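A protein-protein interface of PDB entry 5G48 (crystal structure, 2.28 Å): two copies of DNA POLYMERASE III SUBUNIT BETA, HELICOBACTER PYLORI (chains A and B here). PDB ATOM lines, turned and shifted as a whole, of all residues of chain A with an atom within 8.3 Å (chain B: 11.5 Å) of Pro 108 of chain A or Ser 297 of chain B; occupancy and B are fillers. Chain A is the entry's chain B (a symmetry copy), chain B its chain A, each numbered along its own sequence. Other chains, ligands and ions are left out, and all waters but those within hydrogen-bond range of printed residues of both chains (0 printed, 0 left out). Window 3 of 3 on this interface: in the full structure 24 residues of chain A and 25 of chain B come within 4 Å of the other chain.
Of chain B, only Ser 297 and Glu 298 come within 4 Å of Pro 108 of chain A.
Ser 297 of chain B touches just these residues of chain A: Lys 106 (3.8 Å) and Pro 108 (3.5 Å).
No residue of chain B comes within 4 Å of Thr 69 of chain A.
Ser 95 of chain A touches none of the printed residues of chain B.
Of chain B, only Leu 274 and Glu 298 come within 4 Å of Leu 107 of chain A.
Met 109 of chain A touches none of the printed residues of chain B.
No residue of chain B comes within 4 Å of Phe 110 of chain A.
Printed residues of chain A within 4 Å of Ala 300 of chain B: Phe 105 (3.4 Å).
Printed residues of chain B within 4 Å of Lys 106 of chain A: Ser 297, Glu 298 and Thr 299.
Ser 275 of chain B touches none of the printed residues of chain A.
The nearest residue of chain A that does not touch Ser 297 of chain B is Leu 107 of chain A (4.1 Å).
NZ of Lys 74 of chain A lies within salt-bridge range of OE2 of Glu 298 of chain B (3.9 Å).
The backbone carbonyl oxygen (O) of Thr 299 of chain B lies within hydrogen-bond range of the backbone NH (N) of Lys 106 of chain A (3.0 Å).
Of the 24 printed residues of chain A, 5 touch a printed residue of chain B.
Of the 14 printed residues of chain B, 5 touch a printed residue of chain A.
Printed residues of chain B that touch a printed residue of chain A: Leu 274, Ser 297, Glu 298, Thr 299 and Ala 300.
Hydrophobic or aromatic side chains of chain B that line the printed part of chain A: Leu 274 and Ala 300.
Among the printed residues, Asp or Glu carboxylates within 4 Å of a Lys or Arg side-chain nitrogen of the other chain: Lys 74 of chain A with Glu 298 of chain B.
Lys 74 of chain A touches Leu 274 of chain B.
Phe 105 of chain A touches Thr 299 of chain B (CA to O, 3.1 Å).
Phe 105 of chain A touches Ala 300 of chain B (CD2 to CB, 3.4 Å).
O of Ser 297 of chain B touches O of Lys 106 of chain A (3.8 Å).
Lys 106 of chain A touches Glu 298 of chain B (O to CA, 3.5 Å).
Leu 274 of chain B touches Leu 107 of chain A (CD2 to CD2, 3.9 Å).
Glu 298 of chain B touches Leu 107 of chain A.
Pro 108 of chain A touches Ser 297 of chain B.
Pro 108 of chain A touches Glu 298 of chain B.
The backbone NH (N) of Ser 291 of chain B lies within hydrogen-bond range of the backbone carbonyl oxygen (O) of Ala 300 of chain B, 2.9 Å away.
OG of Ser 294 of chain B lies within hydrogen-bond range of O of Glu 298 of chain B (2.9 Å).
The side-chain amide oxygen of Asn 71 of chain A sits at hydrogen-bond distance from the backbone NH of Lys 74 of chain A (3.0 Å).
The side-chain hydroxyl (OG) of Ser 95 of chain A sits close to the backbone carbonyl oxygen (O) of Leu 107 of chain A.
The backbone NH (N) of Leu 96 of chain A is in hydrogen-bond range of the backbone carbonyl oxygen (O) of Leu 107 of chain A.
No position is printed for both chains.
Of the 11 pairs that touch across the chains among the printed residues, none has its exchanged pair printed and touching as well.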
ATOM      1  N   ALA A  26       4.362  -6.175 -17.193  1.00  0.00           N
ATOM      2  CA  ALA A  26       5.518  -7.071 -17.268  1.00  0.00           C
ATOM      3  C   ALA A  26       6.148  -7.371 -15.906  1.00  0.00           C
ATOM      4  O   ALA A  26       6.858  -8.364 -15.775  1.00  0.00           O
ATOM      5  CB  ALA A  26       6.566  -6.496 -18.213  1.00  0.00           C
ATOM      6  N   SER A  27       5.899  -6.514 -14.911  1.00  0.00           N
ATOM      7  CA  SER A  27       6.411  -6.706 -13.546  1.00  0.00           C
ATOM      8  C   SER A  27       5.580  -7.680 -12.685  1.00  0.00           C
ATOM      9  O   SER A  27       6.010  -8.048 -11.594  1.00  0.00           O
ATOM     10  CB  SER A  27       6.528  -5.349 -12.838  1.00  0.00           C
ATOM     11  OG  SER A  27       5.256  -4.826 -12.492  1.00  0.00           O
ATOM     12  N   HIS A  32       4.296 -13.994 -16.650  1.00  0.00           N
ATOM     13  CA  HIS A  32       5.369 -14.989 -16.751  1.00  0.00           C
ATOM     14  C   HIS A  32       4.847 -16.382 -17.066  1.00  0.00           C
ATOM     15  O   HIS A  32       3.689 -16.693 -16.806  1.00  0.00           O
ATOM     16  CB  HIS A  32       6.210 -15.024 -15.468  1.00  0.00           C
ATOM     17  CG  HIS A  32       7.257 -13.959 -15.412  1.00  0.00           C
ATOM     18  ND1 HIS A  32       8.533 -14.192 -14.951  1.00  0.00           N
ATOM     19  CD2 HIS A  32       7.224 -12.661 -15.791  1.00  0.00           C
ATOM     20  CE1 HIS A  32       9.237 -13.078 -15.032  1.00  0.00           C
ATOM     21  NE2 HIS A  32       8.468 -12.135 -15.545  1.00  0.00           N
ATOM     22  N   ILE A  33       5.731 -17.192 -17.645  1.00  0.00           N
ATOM     23  CA  ILE A  33       5.530 -18.626 -17.832  1.00  0.00           C
ATOM     24  C   ILE A  33       6.370 -19.337 -16.769  1.00  0.00           C
ATOM     25  O   ILE A  33       7.547 -19.022 -16.597  1.00  0.00           O
ATOM     26  CB  ILE A  33       5.961 -19.070 -19.257  1.00  0.00           C
ATOM     27  CG1 ILE A  33       4.970 -18.525 -20.298  1.00  0.00           C
ATOM     28  CG2 ILE A  33       6.068 -20.590 -19.369  1.00  0.00           C
ATOM     29  CD1 ILE A  33       5.482 -18.549 -21.727  1.00  0.00           C
ATOM     30  N   LEU A  35       8.497 -22.421 -15.554  1.00  0.00           N
ATOM     31  CA  LEU A  35       9.384 -23.371 -16.224  1.00  0.00           C
ATOM     32  C   LEU A  35       9.805 -24.462 -15.241  1.00  0.00           C
ATOM     33  O   LEU A  35      10.111 -24.166 -14.084  1.00  0.00           O
ATOM     34  CB  LEU A  35      10.633 -22.657 -16.734  1.00  0.00           C
ATOM     35  CG  LEU A  35      10.445 -21.483 -17.694  1.00  0.00           C
ATOM     36  CD1 LEU A  35      11.766 -20.740 -17.860  1.00  0.00           C
ATOM     37  CD2 LEU A  35       9.908 -21.952 -19.040  1.00  0.00           C
ATOM     38  N   GLY A  68      11.834 -22.400 -12.430  1.00  0.00           N
ATOM     39  CA  GLY A  68      12.075 -20.997 -12.756  1.00  0.00           C
ATOM     40  C   GLY A  68      10.865 -20.371 -13.427  1.00  0.00           C
ATOM     41  O   GLY A  68       9.852 -21.040 -13.642  1.00  0.00           O
ATOM     42  N   THR A  69      10.963 -19.077 -13.718  1.00  0.00           N
ATOM     43  CA  THR A  69       9.930 -18.342 -14.454  1.00  0.00           C
ATOM     44  C   THR A  69      10.591 -17.370 -15.430  1.00  0.00           C
ATOM     45  O   THR A  69      11.776 -17.064 -15.310  1.00  0.00           O
ATOM     46  CB  THR A  69       8.961 -17.537 -13.539  1.00  0.00           C
ATOM     47  OG1 THR A  69       9.497 -16.234 -13.277  1.00  0.00           O
ATOM     48  CG2 THR A  69       8.672 -18.255 -12.210  1.00  0.00           C
ATOM     49  N   ILE A  70       9.804 -16.883 -16.383  1.00  0.00           N
ATOM     50  CA  ILE A  70      10.277 -15.909 -17.372  1.00  0.00           C
ATOM     51  C   ILE A  70       9.099 -15.202 -18.047  1.00  0.00           C
ATOM     52  O   ILE A  70       8.060 -15.819 -18.296  1.00  0.00           O
ATOM     53  CB  ILE A  70      11.158 -16.587 -18.449  1.00  0.00           C
ATOM     54  CG1 ILE A  70      11.831 -15.544 -19.346  1.00  0.00           C
ATOM     55  CG2 ILE A  70      10.351 -17.583 -19.285  1.00  0.00           C
ATOM     56  CD1 ILE A  70      13.013 -16.107 -20.106  1.00  0.00           C
ATOM     57  N   ASN A  71       9.270 -13.912 -18.337  1.00  0.00           N
ATOM     58  CA  ASN A  71       8.260 -13.141 -19.066  1.00  0.00           C
ATOM     59  C   ASN A  71       8.000 -13.781 -20.424  1.00  0.00           C
ATOM     60  O   ASN A  71       8.882 -13.811 -21.273  1.00  0.00           O
ATOM     61  CB  ASN A  71       8.701 -11.685 -19.246  1.00  0.00           C
ATOM     62  CG  ASN A  71       7.629 -10.830 -19.887  1.00  0.00           C
ATOM     63  OD1 ASN A  71       7.442 -10.859 -21.103  1.00  0.00           O
ATOM     64  ND2 ASN A  71       6.918 -10.059 -19.069  1.00  0.00           N
ATOM     65  N   GLY A  72       6.781 -14.284 -20.606  1.00  0.00           N
ATOM     66  CA  GLY A  72       6.416 -15.076 -21.773  1.00  0.00           C
ATOM     67  C   GLY A  72       6.464 -14.345 -23.098  1.00  0.00           C
ATOM     68  O   GLY A  72       6.869 -14.931 -24.101  1.00  0.00           O
ATOM     69  N   LYS A  74       8.346 -11.532 -23.893  1.00  0.00           N
ATOM     70  CA  LYS A  74       9.755 -11.297 -24.200  1.00  0.00           C
ATOM     71  C   LYS A  74      10.478 -12.584 -24.613  1.00  0.00           C
ATOM     72  O   LYS A  74      11.355 -12.550 -25.483  1.00  0.00           O
ATOM     73  CB  LYS A  74      10.466 -10.655 -23.013  1.00  0.00           C
ATOM     74  CG  LYS A  74       9.994  -9.244 -22.717  1.00  0.00           C
ATOM     75  CD  LYS A  74      10.682  -8.660 -21.493  1.00  0.00           C
ATOM     76  CE  LYS A  74      10.324  -7.187 -21.311  1.00  0.00           C
ATOM     77  NZ  LYS A  74       9.026  -7.032 -20.611  1.00  0.00           N
ATOM     78  N   LYS A  92      20.968 -18.386 -13.689  1.00  0.00           N
ATOM     79  CA  LYS A  92      22.090 -17.701 -13.046  1.00  0.00           C
ATOM     80  C   LYS A  92      21.559 -16.862 -11.874  1.00  0.00           C
ATOM     81  O   LYS A  92      21.608 -15.631 -11.923  1.00  0.00           O
ATOM     82  CB  LYS A  92      22.798 -16.787 -14.060  1.00  0.00           C
ATOM     83  CG  LYS A  92      23.756 -17.473 -15.025  1.00  0.00           C
ATOM     84  CD  LYS A  92      23.751 -16.801 -16.391  1.00  0.00           C
ATOM     85  CE  LYS A  92      25.030 -17.064 -17.171  1.00  0.00           C
ATOM     86  NZ  LYS A  92      25.397 -18.510 -17.224  1.00  0.00           N
ATOM     87  N   ASP A  93      21.049 -17.534 -10.838  1.00  0.00           N
ATOM     88  CA  ASP A  93      20.413 -16.879  -9.676  1.00  0.00           C
ATOM     89  C   ASP A  93      19.298 -15.903 -10.092  1.00  0.00           C
ATOM     90  O   ASP A  93      19.569 -14.734 -10.380  1.00  0.00           O
ATOM     91  CB  ASP A  93      21.446 -16.131  -8.803  1.00  0.00           C
ATOM     92  CG  ASP A  93      22.445 -17.059  -8.110  1.00  0.00           C
ATOM     93  OD1 ASP A  93      22.131 -18.245  -7.851  1.00  0.00           O
ATOM     94  OD2 ASP A  93      23.557 -16.576  -7.801  1.00  0.00           O
ATOM     95  N   ASP A  94      18.055 -16.390 -10.105  1.00  0.00           N
ATOM     96  CA  ASP A  94      16.864 -15.622 -10.530  1.00  0.00           C
ATOM     97  C   ASP A  94      17.046 -14.770 -11.810  1.00  0.00           C
ATOM     98  O   ASP A  94      16.590 -13.627 -11.906  1.00  0.00           O
ATOM     99  CB  ASP A  94      16.253 -14.819  -9.355  1.00  0.00           C
ATOM    100  CG  ASP A  94      17.244 -13.879  -8.686  1.00  0.00           C
ATOM    101  OD1 ASP A  94      17.557 -12.819  -9.266  1.00  0.00           O
ATOM    102  OD2 ASP A  94      17.704 -14.197  -7.565  1.00  0.00           O
ATOM    103  N   SER A  95      17.703 -15.379 -12.794  1.00  0.00           N
ATOM    104  CA  SER A  95      17.843 -14.831 -14.137  1.00  0.00           C
ATOM    105  C   SER A  95      18.038 -16.005 -15.101  1.00  0.00           C
ATOM    106  O   SER A  95      18.833 -16.898 -14.806  1.00  0.00           O
ATOM    107  CB  SER A  95      19.037 -13.878 -14.198  1.00  0.00           C
ATOM    108  OG  SER A  95      19.331 -13.508 -15.532  1.00  0.00           O
ATOM    109  N   LEU A  96      17.303 -16.019 -16.220  1.00  0.00           N
ATOM    110  CA  LEU A  96      17.470 -17.052 -17.254  1.00  0.00           C
ATOM    111  C   LEU A  96      18.338 -16.521 -18.389  1.00  0.00           C
ATOM    112  O   LEU A  96      17.998 -15.512 -19.009  1.00  0.00           O
ATOM    113  CB  LEU A  96      16.118 -17.522 -17.814  1.00  0.00           C
ATOM    114  CG  LEU A  96      16.172 -18.793 -18.685  1.00  0.00           C
ATOM    115  CD1 LEU A  96      16.321 -20.043 -17.825  1.00  0.00           C
ATOM    116  CD2 LEU A  96      14.951 -18.929 -19.584  1.00  0.00           C
ATOM    117  N   ALA A  97      19.456 -17.201 -18.650  1.00  0.00           N
ATOM    118  CA  ALA A  97      20.302 -16.900 -19.807  1.00  0.00           C
ATOM    119  C   ALA A  97      19.862 -17.760 -20.980  1.00  0.00           C
ATOM    120  O   ALA A  97      19.602 -18.955 -20.811  1.00  0.00           O
ATOM    121  CB  ALA A  97      21.775 -17.134 -19.502  1.00  0.00           C
ATOM    122  N   PHE A 105      21.207 -13.641 -24.202  1.00  0.00           N
ATOM    123  CA  PHE A 105      20.158 -12.833 -23.590  1.00  0.00           C
ATOM    124  C   PHE A 105      20.060 -13.180 -22.119  1.00  0.00           C
ATOM    125  O   PHE A 105      20.268 -14.333 -21.745  1.00  0.00           O
ATOM    126  CB  PHE A 105      18.800 -13.115 -24.232  1.00  0.00           C
ATOM    127  CG  PHE A 105      18.802 -13.039 -25.729  1.00  0.00           C
ATOM    128  CD1 PHE A 105      19.144 -14.151 -26.489  1.00  0.00           C
ATOM    129  CD2 PHE A 105      18.455 -11.860 -26.385  1.00  0.00           C
ATOM    130  CE1 PHE A 105      19.147 -14.093 -27.872  1.00  0.00           C
ATOM    131  CE2 PHE A 105      18.456 -11.796 -27.768  1.00  0.00           C
ATOM    132  CZ  PHE A 105      18.801 -12.915 -28.513  1.00  0.00           C
ATOM    133  N   LYS A 106      19.749 -12.179 -21.301  1.00  0.00           N
ATOM    134  CA  LYS A 106      19.370 -12.383 -19.911  1.00  0.00           C
ATOM    135  C   LYS A 106      17.962 -11.840 -19.729  1.00  0.00           C
ATOM    136  O   LYS A 106      17.634 -10.764 -20.241  1.00  0.00           O
ATOM    137  CB  LYS A 106      20.333 -11.661 -18.965  1.00  0.00           C
ATOM    138  CG  LYS A 106      21.704 -12.310 -18.856  1.00  0.00           C
ATOM    139  CD  LYS A 106      22.503 -11.735 -17.690  1.00  0.00           C
ATOM    140  CE  LYS A 106      23.717 -12.587 -17.324  1.00  0.00           C
ATOM    141  NZ  LYS A 106      24.974 -12.142 -17.991  1.00  0.00           N
ATOM    142  N   LEU A 107      17.126 -12.604 -19.033  1.00  0.00           N
ATOM    143  CA  LEU A 107      15.832 -12.125 -18.555  1.00  0.00           C
ATOM    144  C   LEU A 107      15.673 -12.510 -17.078  1.00  0.00           C
ATOM    145  O   LEU A 107      16.160 -13.567 -16.669  1.00  0.00           O
ATOM    146  CB  LEU A 107      14.693 -12.699 -19.405  1.00  0.00           C
ATOM    147  CG  LEU A 107      14.470 -12.024 -20.766  1.00  0.00           C
ATOM    148  CD1 LEU A 107      13.501 -12.829 -21.617  1.00  0.00           C
ATOM    149  CD2 LEU A 107      13.977 -10.588 -20.597  1.00  0.00           C
ATOM    150  N   PRO A 108      15.011 -11.647 -16.276  1.00  0.00           N
ATOM    151  CA  PRO A 108      14.833 -11.923 -14.852  1.00  0.00           C
ATOM    152  C   PRO A 108      13.726 -12.938 -14.594  1.00  0.00           C
ATOM    153  O   PRO A 108      12.711 -12.945 -15.298  1.00  0.00           O
ATOM    154  CB  PRO A 108      14.428 -10.565 -14.288  1.00  0.00           C
ATOM    155  CG  PRO A 108      13.660  -9.932 -15.404  1.00  0.00           C
ATOM    156  CD  PRO A 108      14.344 -10.388 -16.666  1.00  0.00           C
ATOM    157  N   MET A 109      13.934 -13.781 -13.586  1.00  0.00           N
ATOM    158  CA  MET A 109      12.939 -14.749 -13.131  1.00  0.00           C
ATOM    159  C   MET A 109      12.296 -14.239 -11.845  1.00  0.00           C
ATOM    160  O   MET A 109      12.905 -13.459 -11.104  1.00  0.00           O
ATOM    161  CB  MET A 109      13.597 -16.104 -12.858  1.00  0.00           C
ATOM    162  CG  MET A 109      14.512 -16.581 -13.972  1.00  0.00           C
ATOM    163  SD  MET A 109      14.640 -18.373 -14.058  1.00  0.00           S
ATOM    164  CE  MET A 109      15.454 -18.721 -12.496  1.00  0.00           C
ATOM    165  N   PHE A 110      11.070 -14.687 -11.591  1.00  0.00           N
ATOM    166  CA  PHE A 110      10.372 -14.394 -10.339  1.00  0.00           C
ATOM    167  C   PHE A 110      10.352 -15.636  -9.459  1.00  0.00           C
ATOM    168  O   PHE A 110      10.883 -16.683  -9.833  1.00  0.00           O
ATOM    169  CB  PHE A 110       8.946 -13.892 -10.622  1.00  0.00           C
ATOM    170  CG  PHE A 110       8.877 -12.566 -11.351  1.00  0.00           C
ATOM    171  CD1 PHE A 110       9.893 -11.605 -11.256  1.00  0.00           C
ATOM    172  CD2 PHE A 110       7.751 -12.256 -12.105  1.00  0.00           C
ATOM    173  CE1 PHE A 110       9.791 -10.391 -11.926  1.00  0.00           C
ATOM    174  CE2 PHE A 110       7.646 -11.041 -12.770  1.00  0.00           C
ATOM    175  CZ  PHE A 110       8.665 -10.109 -12.680  1.00  0.00           C
ATOM    176  N   ASP A 111       9.776 -15.506  -8.271  1.00  0.00           N
ATOM    177  CA  ASP A 111       9.608 -16.647  -7.387  1.00  0.00           C
ATOM    178  C   ASP A 111       8.599 -17.615  -8.007  1.00  0.00           C
ATOM    179  O   ASP A 111       7.458 -17.237  -8.289  1.00  0.00           O
ATOM    180  CB  ASP A 111       9.145 -16.199  -5.998  1.00  0.00           C
ATOM    181  CG  ASP A 111       9.211 -17.314  -4.972  1.00  0.00           C
ATOM    182  OD1 ASP A 111       9.246 -18.506  -5.358  1.00  0.00           O
ATOM    183  OD2 ASP A 111       9.232 -16.995  -3.765  1.00  0.00           O
ATOM    184  N   SER B 273      14.424  -6.873 -29.744  1.00  0.00           N
ATOM    185  CA  SER B 273      13.463  -7.664 -28.964  1.00  0.00           C
ATOM    186  C   SER B 273      13.264  -7.159 -27.526  1.00  0.00           C
ATOM    187  O   SER B 273      12.177  -7.315 -26.975  1.00  0.00           O
ATOM    188  CB  SER B 273      13.886  -9.136 -28.922  1.00  0.00           C
ATOM    189  OG  SER B 273      15.123  -9.295 -28.246  1.00  0.00           O
ATOM    190  N   LEU B 274      14.306  -6.576 -26.928  1.00  0.00           N
ATOM    191  CA  LEU B 274      14.236  -6.023 -25.565  1.00  0.00           C
ATOM    192  C   LEU B 274      14.424  -4.508 -25.447  1.00  0.00           C
ATOM    193  O   LEU B 274      14.274  -3.964 -24.352  1.00  0.00           O
ATOM    194  CB  LEU B 274      15.273  -6.711 -24.674  1.00  0.00           C
ATOM    195  CG  LEU B 274      15.146  -8.231 -24.575  1.00  0.00           C
ATOM    196  CD1 LEU B 274      16.275  -8.781 -23.718  1.00  0.00           C
ATOM    197  CD2 LEU B 274      13.786  -8.619 -24.015  1.00  0.00           C
ATOM    198  N   SER B 275      14.743  -3.826 -26.544  1.00  0.00           N
ATOM    199  CA  SER B 275      15.016  -2.388 -26.501  1.00  0.00           C
ATOM    200  C   SER B 275      14.567  -1.694 -27.772  1.00  0.00           C
ATOM    201  O   SER B 275      14.344  -2.338 -28.796  1.00  0.00           O
ATOM    202  CB  SER B 275      16.517  -2.164 -26.316  1.00  0.00           C
ATOM    203  OG  SER B 275      17.238  -2.767 -27.379  1.00  0.00           O
ATOM    204  N   SER B 291      21.576  -4.405 -26.490  1.00  0.00           N
ATOM    205  CA  SER B 291      20.417  -3.605 -26.076  1.00  0.00           C
ATOM    206  C   SER B 291      20.882  -2.527 -25.089  1.00  0.00           C
ATOM    207  O   SER B 291      21.737  -2.784 -24.246  1.00  0.00           O
ATOM    208  CB  SER B 291      19.322  -4.491 -25.463  1.00  0.00           C
ATOM    209  OG  SER B 291      19.782  -5.197 -24.321  1.00  0.00           O
ATOM    210  N   LEU B 292      20.328  -1.323 -25.228  1.00  0.00           N
ATOM    211  CA  LEU B 292      20.844  -0.123 -24.560  1.00  0.00           C
ATOM    212  C   LEU B 292      19.830   0.475 -23.589  1.00  0.00           C
ATOM    213  O   LEU B 292      20.137   0.642 -22.409  1.00  0.00           O
ATOM    214  CB  LEU B 292      21.241   0.911 -25.612  1.00  0.00           C
ATOM    215  CG  LEU B 292      21.821   2.245 -25.141  1.00  0.00           C
ATOM    216  CD1 LEU B 292      23.101   2.037 -24.341  1.00  0.00           C
ATOM    217  CD2 LEU B 292      22.065   3.131 -26.351  1.00  0.00           C
ATOM    218  N   ASP B 293      18.633   0.798 -24.085  1.00  0.00           N
ATOM    219  CA  ASP B 293      17.520   1.240 -23.221  1.00  0.00           C
ATOM    220  C   ASP B 293      16.587   0.084 -22.801  1.00  0.00           C
ATOM    221  O   ASP B 293      15.399   0.297 -22.527  1.00  0.00           O
ATOM    222  CB  ASP B 293      16.749   2.439 -23.841  1.00  0.00           C
ATOM    223  CG  ASP B 293      15.874   2.066 -25.048  1.00  0.00           C
ATOM    224  OD1 ASP B 293      15.775   0.878 -25.423  1.00  0.00           O
ATOM    225  OD2 ASP B 293      15.280   2.995 -25.638  1.00  0.00           O
ATOM    226  N   SER B 294      17.130  -1.136 -22.754  1.00  0.00           N
ATOM    227  CA  SER B 294      16.446  -2.266 -22.129  1.00  0.00           C
ATOM    228  C   SER B 294      16.321  -2.020 -20.623  1.00  0.00           C
ATOM    229  O   SER B 294      17.064  -1.217 -20.045  1.00  0.00           O
ATOM    230  CB  SER B 294      17.187  -3.585 -22.408  1.00  0.00           C
ATOM    231  OG  SER B 294      18.577  -3.479 -22.140  1.00  0.00           O
ATOM    232  N   GLU B 295      15.377  -2.720 -20.001  1.00  0.00           N
ATOM    233  CA  GLU B 295      15.036  -2.512 -18.590  1.00  0.00           C
ATOM    234  C   GLU B 295      16.117  -3.112 -17.686  1.00  0.00           C
ATOM    235  O   GLU B 295      17.052  -3.763 -18.164  1.00  0.00           O
ATOM    236  CB  GLU B 295      13.667  -3.138 -18.264  1.00  0.00           C
ATOM    237  CG  GLU B 295      12.492  -2.639 -19.113  1.00  0.00           C
ATOM    238  CD  GLU B 295      11.769  -1.420 -18.548  1.00  0.00           C
ATOM    239  OE1 GLU B 295      11.645  -1.289 -17.311  1.00  0.00           O
ATOM    240  OE2 GLU B 295      11.290  -0.597 -19.360  1.00  0.00           O
ATOM    241  N   HIS B 296      15.980  -2.877 -16.382  1.00  0.00           N
ATOM    242  CA  HIS B 296      16.911  -3.403 -15.375  1.00  0.00           C
ATOM    243  C   HIS B 296      16.983  -4.936 -15.484  1.00  0.00           C
ATOM    244  O   HIS B 296      15.951  -5.605 -15.451  1.00  0.00           O
ATOM    245  CB  HIS B 296      16.456  -2.997 -13.956  1.00  0.00           C
ATOM    246  CG  HIS B 296      17.578  -2.702 -13.006  1.00  0.00           C
ATOM    247  ND1 HIS B 296      17.407  -1.914 -11.885  1.00  0.00           N
ATOM    248  CD2 HIS B 296      18.882  -3.073 -13.006  1.00  0.00           C
ATOM    249  CE1 HIS B 296      18.552  -1.821 -11.233  1.00  0.00           C
ATOM    250  NE2 HIS B 296      19.464  -2.513 -11.893  1.00  0.00           N
ATOM    251  N   SER B 297      18.196  -5.468 -15.645  1.00  0.00           N
ATOM    252  CA  SER B 297      18.452  -6.919 -15.758  1.00  0.00           C
ATOM    253  C   SER B 297      17.806  -7.613 -16.977  1.00  0.00           C
ATOM    254  O   SER B 297      17.496  -8.808 -16.928  1.00  0.00           O
ATOM    255  CB  SER B 297      18.094  -7.651 -14.448  1.00  0.00           C
ATOM    256  OG  SER B 297      16.697  -7.817 -14.287  1.00  0.00           O
ATOM    257  N   GLU B 298      17.623  -6.863 -18.064  1.00  0.00           N
ATOM    258  CA  GLU B 298      17.248  -7.427 -19.354  1.00  0.00           C
ATOM    259  C   GLU B 298      18.328  -7.038 -20.351  1.00  0.00           C
ATOM    260  O   GLU B 298      18.660  -5.858 -20.477  1.00  0.00           O
ATOM    261  CB  GLU B 298      15.892  -6.902 -19.810  1.00  0.00           C
ATOM    262  CG  GLU B 298      14.764  -7.220 -18.840  1.00  0.00           C
ATOM    263  CD  GLU B 298      13.386  -6.962 -19.415  1.00  0.00           C
ATOM    264  OE1 GLU B 298      13.291  -6.388 -20.524  1.00  0.00           O
ATOM    265  OE2 GLU B 298      12.392  -7.340 -18.753  1.00  0.00           O
ATOM    266  N   THR B 299      18.882  -8.035 -21.040  1.00  0.00           N
ATOM    267  CA  THR B 299      19.998  -7.830 -21.964  1.00  0.00           C
ATOM    268  C   THR B 299      19.828  -8.691 -23.211  1.00  0.00           C
ATOM    269  O   THR B 299      19.357  -9.826 -23.133  1.00  0.00           O
ATOM    270  CB  THR B 299      21.340  -8.172 -21.289  1.00  0.00           C
ATOM    271  OG1 THR B 299      21.442  -7.468 -20.049  1.00  0.00           O
ATOM    272  CG2 THR B 299      22.523  -7.785 -22.170  1.00  0.00           C
ATOM    273  N   ALA B 300      20.193  -8.125 -24.359  1.00  0.00           N
ATOM    274  CA  ALA B 300      20.260  -8.854 -25.620  1.00  0.00           C
ATOM    275  C   ALA B 300      21.577  -8.502 -26.286  1.00  0.00           C
ATOM    276  O   ALA B 300      21.828  -7.338 -26.563  1.00  0.00           O
ATOM    277  CB  ALA B 300      19.096  -8.480 -26.515  1.00  0.00           C
ATOM    278  N   LYS B 301      22.422  -9.507 -26.504  1.00  0.00           N
ATOM    279  CA  LYS B 301      23.713  -9.330 -27.161  1.00  0.00           C
ATOM    280  C   LYS B 301      23.845 -10.270 -28.342  1.00  0.00           C
ATOM    281  O   LYS B 301      23.338 -11.392 -28.318  1.00  0.00           O
ATOM    282  CB  LYS B 301      24.864  -9.625 -26.201  1.00  0.00           C
ATOM    283  CG  LYS B 301      25.026  -8.623 -25.075  1.00  0.00           C
ATOM    284  CD  LYS B 301      26.121  -9.042 -24.098  1.00  0.00           C
ATOM    285  CE  LYS B 301      27.500  -9.043 -24.742  1.00  0.00           C
ATOM    286  NZ  LYS B 301      28.599  -9.098 -23.736  1.00  0.00           N
